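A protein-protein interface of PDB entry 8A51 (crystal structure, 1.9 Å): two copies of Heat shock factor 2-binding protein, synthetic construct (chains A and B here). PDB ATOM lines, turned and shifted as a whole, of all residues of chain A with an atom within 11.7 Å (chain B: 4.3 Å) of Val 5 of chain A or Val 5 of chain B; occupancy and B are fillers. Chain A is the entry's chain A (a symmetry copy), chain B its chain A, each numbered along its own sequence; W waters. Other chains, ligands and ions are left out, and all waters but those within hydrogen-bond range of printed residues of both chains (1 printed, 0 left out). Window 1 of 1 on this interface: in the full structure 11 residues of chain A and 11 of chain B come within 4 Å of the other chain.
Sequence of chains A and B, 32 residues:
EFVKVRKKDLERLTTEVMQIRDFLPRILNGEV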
ATOM      1  N   GLU A   1      21.458  11.420 -18.777  1.00  0.00           N
ATOM      2  CA  GLU A   1      20.186  10.871 -19.256  1.00  0.00           C
ATOM      3  C   GLU A   1      20.396   9.572 -20.045  1.00  0.00           C
ATOM      4  O   GLU A   1      21.176   9.537 -21.001  1.00  0.00           O
ATOM      5  CB  GLU A   1      19.436  11.906 -20.120  1.00  0.00           C
ATOM      6  CG  GLU A   1      18.106  11.410 -20.671  1.00  0.00           C
ATOM      7  CD  GLU A   1      17.247  12.456 -21.358  1.00  0.00           C
ATOM      8  OE1 GLU A   1      16.183  12.080 -21.902  1.00  0.00           O
ATOM      9  OE2 GLU A   1      17.637  13.645 -21.363  1.00  0.00           O
ATOM     10  N   PHE A   2      19.675   8.516 -19.650  1.00  0.00           N
ATOM     11  CA  PHE A   2      19.723   7.211 -20.295  1.00  0.00           C
ATOM     12  C   PHE A   2      18.398   6.895 -20.982  1.00  0.00           C
ATOM     13  O   PHE A   2      17.346   7.365 -20.555  1.00  0.00           O
ATOM     14  CB  PHE A   2      20.023   6.112 -19.263  1.00  0.00           C
ATOM     15  CG  PHE A   2      21.469   6.031 -18.828  1.00  0.00           C
ATOM     16  CD1 PHE A   2      21.986   6.932 -17.914  1.00  0.00           C
ATOM     17  CD2 PHE A   2      22.294   5.022 -19.293  1.00  0.00           C
ATOM     18  CE1 PHE A   2      23.312   6.851 -17.510  1.00  0.00           C
ATOM     19  CE2 PHE A   2      23.613   4.930 -18.870  1.00  0.00           C
ATOM     20  CZ  PHE A   2      24.114   5.846 -17.987  1.00  0.00           C
ATOM     21  N   VAL A   3      18.468   6.074 -22.039  1.00  0.00           N
ATOM     22  CA  VAL A   3      17.342   5.556 -22.813  1.00  0.00           C
ATOM     23  C   VAL A   3      17.450   4.021 -22.813  1.00  0.00           C
ATOM     24  O   VAL A   3      18.536   3.469 -22.617  1.00  0.00           O
ATOM     25  CB  VAL A   3      17.278   6.122 -24.260  1.00  0.00           C
ATOM     26  CG1 VAL A   3      17.104   7.635 -24.262  1.00  0.00           C
ATOM     27  CG2 VAL A   3      18.486   5.709 -25.100  1.00  0.00           C
ATOM     28  N   LYS A   4      16.326   3.342 -23.032  1.00  0.00           N
ATOM     29  CA  LYS A   4      16.251   1.886 -23.065  1.00  0.00           C
ATOM     30  C   LYS A   4      16.335   1.379 -24.526  1.00  0.00           C
ATOM     31  O   LYS A   4      15.741   1.977 -25.425  1.00  0.00           O
ATOM     32  CB  LYS A   4      14.939   1.420 -22.407  1.00  0.00           C
ATOM     33  N   VAL A   5      17.060   0.267 -24.745  1.00  0.00           N
ATOM     34  CA  VAL A   5      17.293  -0.329 -26.065  1.00  0.00           C
ATOM     35  C   VAL A   5      17.182  -1.857 -25.939  1.00  0.00           C
ATOM     36  O   VAL A   5      17.681  -2.412 -24.978  1.00  0.00           O
ATOM     37  CB  VAL A   5      18.714   0.086 -26.580  1.00  0.00           C
ATOM     38  CG1 VAL A   5      19.108  -0.694 -27.832  1.00  0.00           C
ATOM     39  CG2 VAL A   5      18.801   1.590 -26.835  1.00  0.00           C
ATOM     40  N   ARG A   6      16.540  -2.540 -26.897  1.00  0.00           N
ATOM     41  CA  ARG A   6      16.436  -4.001 -26.853  1.00  0.00           C
ATOM     42  C   ARG A   6      17.833  -4.580 -27.093  1.00  0.00           C
ATOM     43  O   ARG A   6      18.523  -4.133 -28.005  1.00  0.00           O
ATOM     44  CB  ARG A   6      15.440  -4.516 -27.897  1.00  0.00           C
ATOM     45  CG  ARG A   6      14.030  -4.061 -27.603  1.00  0.00           C
ATOM     46  CD  ARG A   6      13.060  -4.361 -28.722  1.00  0.00           C
ATOM     47  NE  ARG A   6      11.683  -4.086 -28.310  1.00  0.00           N
ATOM     48  CZ  ARG A   6      10.921  -4.901 -27.579  1.00  0.00           C
ATOM     49  NH1 ARG A   6      11.397  -6.069 -27.152  1.00  0.00           N
ATOM     50  NH2 ARG A   6       9.682  -4.549 -27.257  1.00  0.00           N
ATOM     51  N   LYS A   7      18.255  -5.537 -26.249  1.00  0.00           N
ATOM     52  CA  LYS A   7      19.575  -6.175 -26.327  1.00  0.00           C
ATOM     53  C   LYS A   7      19.788  -6.806 -27.713  1.00  0.00           C
ATOM     54  O   LYS A   7      20.857  -6.643 -28.294  1.00  0.00           O
ATOM     55  CB  LYS A   7      19.707  -7.239 -25.223  1.00  0.00           C
ATOM     56  CG  LYS A   7      21.111  -7.811 -25.028  1.00  0.00           C
ATOM     57  CD  LYS A   7      21.029  -9.117 -24.241  1.00  0.00           C
ATOM     58  CE  LYS A   7      22.375  -9.686 -23.862  1.00  0.00           C
ATOM     59  NZ  LYS A   7      22.232 -10.991 -23.147  1.00  0.00           N
ATOM     60  N   LYS A   8      18.765  -7.490 -28.229  1.00  0.00           N
ATOM     61  CA  LYS A   8      18.795  -8.132 -29.544  1.00  0.00           C
ATOM     62  C   LYS A   8      19.030  -7.110 -30.655  1.00  0.00           C
ATOM     63  O   LYS A   8      19.732  -7.413 -31.617  1.00  0.00           O
ATOM     64  CB  LYS A   8      17.474  -8.867 -29.789  1.00  0.00           C
ATOM     65  CG  LYS A   8      17.432  -9.713 -31.050  1.00  0.00           C
ATOM     66  CD  LYS A   8      16.089 -10.400 -31.176  1.00  0.00           C
ATOM     67  CE  LYS A   8      15.908 -11.081 -32.512  1.00  0.00           C
ATOM     68  NZ  LYS A   8      16.929 -12.135 -32.756  1.00  0.00           N
ATOM     69  N   ASP A   9      18.443  -5.914 -30.532  1.00  0.00           N
ATOM     70  CA  ASP A   9      18.608  -4.853 -31.522  1.00  0.00           C
ATOM     71  C   ASP A   9      20.031  -4.267 -31.437  1.00  0.00           C
ATOM     72  O   ASP A   9      20.614  -3.945 -32.467  1.00  0.00           O
ATOM     73  CB  ASP A   9      17.607  -3.727 -31.287  1.00  0.00           C
ATOM     74  CG  ASP A   9      16.203  -3.975 -31.772  1.00  0.00           C
ATOM     75  OD1 ASP A   9      15.957  -5.051 -32.386  1.00  0.00           O
ATOM     76  OD2 ASP A   9      15.349  -3.087 -31.570  1.00  0.00           O
ATOM     77  N   LEU A  10      20.579  -4.106 -30.221  1.00  0.00           N
ATOM     78  CA  LEU A  10      21.950  -3.638 -30.069  1.00  0.00           C
ATOM     79  C   LEU A  10      22.927  -4.684 -30.619  1.00  0.00           C
ATOM     80  O   LEU A  10      23.959  -4.318 -31.174  1.00  0.00           O
ATOM     81  CB  LEU A  10      22.273  -3.316 -28.601  1.00  0.00           C
ATOM     82  CG  LEU A  10      23.671  -2.758 -28.353  1.00  0.00           C
ATOM     83  CD1 LEU A  10      23.913  -1.477 -29.147  1.00  0.00           C
ATOM     84  CD2 LEU A  10      23.895  -2.495 -26.896  1.00  0.00           C
ATOM     85  N   GLU A  11      22.626  -5.987 -30.446  1.00  0.00           N
ATOM     86  CA  GLU A  11      23.437  -7.071 -31.005  1.00  0.00           C
ATOM     87  C   GLU A  11      23.384  -7.025 -32.537  1.00  0.00           C
ATOM     88  O   GLU A  11      24.388  -7.282 -33.202  1.00  0.00           O
ATOM     89  CB  GLU A  11      22.938  -8.447 -30.525  1.00  0.00           C
ATOM     90  CG  GLU A  11      23.278  -8.754 -29.077  1.00  0.00           C
ATOM     91  CD  GLU A  11      22.591  -9.976 -28.498  1.00  0.00           C
ATOM     92  OE1 GLU A  11      21.927 -10.715 -29.262  1.00  0.00           O
ATOM     93  OE2 GLU A  11      22.714 -10.194 -27.269  1.00  0.00           O
ATOM     94  N   ARG A  12      22.207  -6.732 -33.096  1.00  0.00           N
ATOM     95  CA  ARG A  12      22.053  -6.630 -34.534  1.00  0.00           C
ATOM     96  C   ARG A  12      22.826  -5.423 -35.068  1.00  0.00           C
ATOM     97  O   ARG A  12      23.498  -5.531 -36.085  1.00  0.00           O
ATOM     98  CB  ARG A  12      20.572  -6.523 -34.901  1.00  0.00           C
ATOM     99  CG  ARG A  12      20.318  -6.269 -36.370  1.00  0.00           C
ATOM    100  CD  ARG A  12      20.783  -7.397 -37.284  1.00  0.00           C
ATOM    101  NE  ARG A  12      20.771  -6.982 -38.681  1.00  0.00           N
ATOM    102  CZ  ARG A  12      19.676  -6.856 -39.432  1.00  0.00           C
ATOM    103  NH1 ARG A  12      18.478  -7.092 -38.918  1.00  0.00           N
ATOM    104  NH2 ARG A  12      19.774  -6.460 -40.689  1.00  0.00           N
ATOM    105  N   LEU A  13      22.706  -4.279 -34.408  1.00  0.00           N
ATOM    106  CA  LEU A  13      23.435  -3.071 -34.785  1.00  0.00           C
ATOM    107  C   LEU A  13      24.957  -3.309 -34.748  1.00  0.00           C
ATOM    108  O   LEU A  13      25.673  -2.901 -35.657  1.00  0.00           O
ATOM    109  CB  LEU A  13      23.059  -1.929 -33.831  1.00  0.00           C
ATOM    110  CG  LEU A  13      23.568  -0.534 -34.162  1.00  0.00           C
ATOM    111  CD1 LEU A  13      23.059  -0.040 -35.501  1.00  0.00           C
ATOM    112  CD2 LEU A  13      23.148   0.419 -33.085  1.00  0.00           C
ATOM    113  N   THR A  14      25.420  -4.038 -33.741  1.00  0.00           N
ATOM    114  CA  THR A  14      26.826  -4.426 -33.606  1.00  0.00           C
ATOM    115  C   THR A  14      27.245  -5.289 -34.791  1.00  0.00           C
ATOM    116  O   THR A  14      28.297  -5.057 -35.375  1.00  0.00           O
ATOM    117  CB  THR A  14      27.034  -5.142 -32.268  1.00  0.00           C
ATOM    118  OG1 THR A  14      26.648  -4.235 -31.231  1.00  0.00           O
ATOM    119  CG2 THR A  14      28.475  -5.584 -32.041  1.00  0.00           C
ATOM    120  N   PHE B   2      15.917  -5.592 -22.227  1.00  0.00           N
ATOM    121  CA  PHE B   2      16.386  -4.250 -22.542  1.00  0.00           C
ATOM    122  C   PHE B   2      17.678  -3.936 -21.794  1.00  0.00           C
ATOM    123  O   PHE B   2      17.916  -4.465 -20.711  1.00  0.00           O
ATOM    124  CB  PHE B   2      15.323  -3.206 -22.160  1.00  0.00           C
ATOM    125  CG  PHE B   2      14.162  -3.104 -23.122  1.00  0.00           C
ATOM    126  CD1 PHE B   2      13.144  -4.042 -23.107  1.00  0.00           C
ATOM    127  CD2 PHE B   2      14.062  -2.042 -24.004  1.00  0.00           C
ATOM    128  CE1 PHE B   2      12.074  -3.942 -23.987  1.00  0.00           C
ATOM    129  CE2 PHE B   2      12.980  -1.934 -24.867  1.00  0.00           C
ATOM    130  CZ  PHE B   2      11.998  -2.884 -24.856  1.00  0.00           C
ATOM    131  N   VAL B   3      18.494  -3.051 -22.382  1.00  0.00           N
ATOM    132  CA  VAL B   3      19.743  -2.524 -21.836  1.00  0.00           C
ATOM    133  C   VAL B   3      19.633  -0.989 -21.833  1.00  0.00           C
ATOM    134  O   VAL B   3      18.854  -0.415 -22.598  1.00  0.00           O
ATOM    135  CB  VAL B   3      21.004  -3.003 -22.610  1.00  0.00           C
ATOM    136  CG1 VAL B   3      21.150  -4.518 -22.558  1.00  0.00           C
ATOM    137  CG2 VAL B   3      21.026  -2.501 -24.053  1.00  0.00           C
ATOM    138  N   LYS B   4      20.413  -0.335 -20.974  1.00  0.00           N
ATOM    139  CA  LYS B   4      20.434   1.117 -20.842  1.00  0.00           C
ATOM    140  C   LYS B   4      21.590   1.715 -21.682  1.00  0.00           C
ATOM    141  O   LYS B   4      22.686   1.153 -21.715  1.00  0.00           O
ATOM    142  CB  LYS B   4      20.592   1.499 -19.359  1.00  0.00           C
ATOM    143  N   VAL B   5      21.337   2.860 -22.339  1.00  0.00           N
ATOM    144  CA  VAL B   5      22.290   3.543 -23.221  1.00  0.00           C
ATOM    145  C   VAL B   5      22.196   5.056 -22.967  1.00  0.00           C
ATOM    146  O   VAL B   5      21.102   5.567 -22.822  1.00  0.00           O
ATOM    147  CB  VAL B   5      21.951   3.206 -24.714  1.00  0.00           C
ATOM    148  CG1 VAL B   5      22.753   4.073 -25.682  1.00  0.00           C
ATOM    149  CG2 VAL B   5      22.165   1.724 -25.017  1.00  0.00           C
ATOM    150  N   ARG B   6      23.327   5.774 -22.916  1.00  0.00           N
ATOM    151  CA  ARG B   6      23.300   7.225 -22.717  1.00  0.00           C
ATOM    152  C   ARG B   6      22.712   7.863 -23.978  1.00  0.00           C
ATOM    153  O   ARG B   6      23.107   7.496 -25.081  1.00  0.00           O
ATOM    154  CB  ARG B   6      24.701   7.770 -22.427  1.00  0.00           C
ATOM    155  CG  ARG B   6      25.248   7.253 -21.117  1.00  0.00           C
ATOM    156  CD  ARG B   6      26.706   7.588 -20.903  1.00  0.00           C
ATOM    157  NE  ARG B   6      27.129   7.244 -19.546  1.00  0.00           N
ATOM    158  CZ  ARG B   6      26.912   7.987 -18.459  1.00  0.00           C
ATOM    159  NH1 ARG B   6      26.256   9.142 -18.552  1.00  0.00           N
ATOM    160  NH2 ARG B   6      27.338   7.576 -17.271  1.00  0.00           N
ATOM    161  N   LYS B   7      21.744   8.780 -23.809  1.00  0.00           N
ATOM    162  CA  LYS B   7      21.062   9.466 -24.914  1.00  0.00           C
ATOM    163  C   LYS B   7      22.079  10.185 -25.813  1.00  0.00           C
ATOM    164  O   LYS B   7      21.981  10.093 -27.033  1.00  0.00           O
ATOM    165  CB  LYS B   7      20.032  10.464 -24.354  1.00  0.00           C
ATOM    166  CG  LYS B   7      19.079  11.068 -25.383  1.00  0.00           C
ATOM    167  CD  LYS B   7      18.424  12.322 -24.805  1.00  0.00           C
ATOM    168  CE  LYS B   7      17.349  12.909 -25.685  1.00  0.00           C
ATOM    169  NZ  LYS B   7      16.788  14.164 -25.095  1.00  0.00           N
ATOM    170  N   LEU B  10      23.824   7.670 -28.012  1.00  0.00           N
ATOM    171  CA  LEU B  10      22.957   7.238 -29.100  1.00  0.00           C
ATOM    172  C   LEU B  10      22.844   8.347 -30.154  1.00  0.00           C
ATOM    173  O   LEU B  10      22.751   8.049 -31.340  1.00  0.00           O
ATOM    174  CB  LEU B  10      21.565   6.839 -28.585  1.00  0.00           C
ATOM    175  CG  LEU B  10      20.607   6.313 -29.649  1.00  0.00           C
ATOM    176  CD1 LEU B  10      21.178   5.091 -30.363  1.00  0.00           C
ATOM    177  CD2 LEU B  10      19.278   5.970 -29.052  1.00  0.00           C
HETATM  178  O   HOH W   1      23.144  11.051 -22.157  1.00  0.00           O
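The backbone NH (N) of Val 3 of chain B is in hydrogen-bond range of the backbone carbonyl oxygen (O) of Val 5 of chain A. The backbone carbonyl oxygen (O) of Val 5 of chain B is in hydrogen-bond range of the backbone NH (N) of Val 3 of chain A (2.8 Å). NZ of Lys 7 of chain B is in salt-bridge range of OE1 of Glu 1 of chain A, 3.9 Å away.
CA of Arg 6 of chain B touches O of Glu 1 of chain A, at 3.6 Å. Phe 2 of chain A touches Lys 4 of chain B (CD2 to CB, 3.9 Å). CZ of Arg 6 of chain B touches CZ of Phe 2 of chain A, at 3.6 Å. Val 3 of chain A touches Val 3 of chain B. O of Val 3 of chain A touches CA of Lys 4 of chain B, at 3.5 Å. Phe 2 of chain B touches Lys 4 of chain A. O of Val 3 of chain B touches CA of Lys 4 of chain A, at 3.5 Å. Val 5 of chain A touches Phe 2 of chain B. Val 5 of chain A touches Val 5 of chain B. Arg 6 of chain A touches Phe 2 of chain B (CZ to CZ, 3.6 Å).
Of the printed residues of chain B, Val 3 of chain A touches Val 3 (3.9 Å), Lys 4 (3.5 Å) and Val 5 (2.8 Å). Printed residues of chain B within 4 Å of Lys 4 of chain A: Phe 2 (3.9 Å) and Val 3 (3.5 Å). Of the printed residues of chain B, Val 5 of chain A touches Phe 2, Val 3 and Val 5. Lys 7 of chain A touches none of the printed residues of chain B. Leu 13 of chain A touches none of the printed residues of chain B. Of chain A, only Phe 2 and Val 3 come within 4 Å of Lys 4 of chain B. Of chain A, only Phe 2 (3.3 Å), Val 3 (2.8 Å) and Val 5 (3.8 Å) come within 4 Å of Val 5 of chain B. Of the printed residues of chain A, Arg 6 of chain B touches Glu 1 (3.6 Å) and Phe 2 (3.6 Å). Printed residues of chain A within 4 Å of Lys 7 of chain B: Glu 1. Leu 10 of chain B touches none of the printed residues of chain A. The nearest printed residue of chain B that does not touch Val 5 of chain A is Leu 10 of chain B (4.9 Å). The nearest residue of chain A that does not touch Val 5 of chain B is Glu 1 of chain A (4.4 Å). The nearest printed residue of chain B that does not touch Phe 2 of chain A is Lys 7 of chain B (4.3 Å).
Of the 14 printed residues of chain A, 6 touch a printed residue of chain B. Of the 7 printed residues of chain B, 6 touch a printed residue of chain A. Hydrophobic or aromatic side chains of chain B that line the printed part of chain A: Phe 2, Val 3 and Val 5. Among the printed residues, 14 pairs touch across the chains.
Phe 2 of chain A touches Lys 4 of chain B, and with the chains exchanged Lys 4 of chain A touches Phe 2 of chain B. Phe 2 of chain A touches Val 5 of chain B, and with the chains exchanged Val 5 of chain A touches Phe 2 of chain B. Phe 2 of chain A touches Arg 6 of chain B, and with the chains exchanged Arg 6 of chain A touches Phe 2 of chain B. Val 5 of chain B touches its own counterpart, Val 5 of chain A. Of the 14 pairs that touch across the chains among the printed residues, 12 have their exchanged pair printed and touching as well.
Water W1 lies within hydrogen-bond range of the backbone carbonyl oxygen (O) of Glu 1 of chain A (2.7 Å) and the backbone NH (N) of Lys 7 of chain B (3.1 Å).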
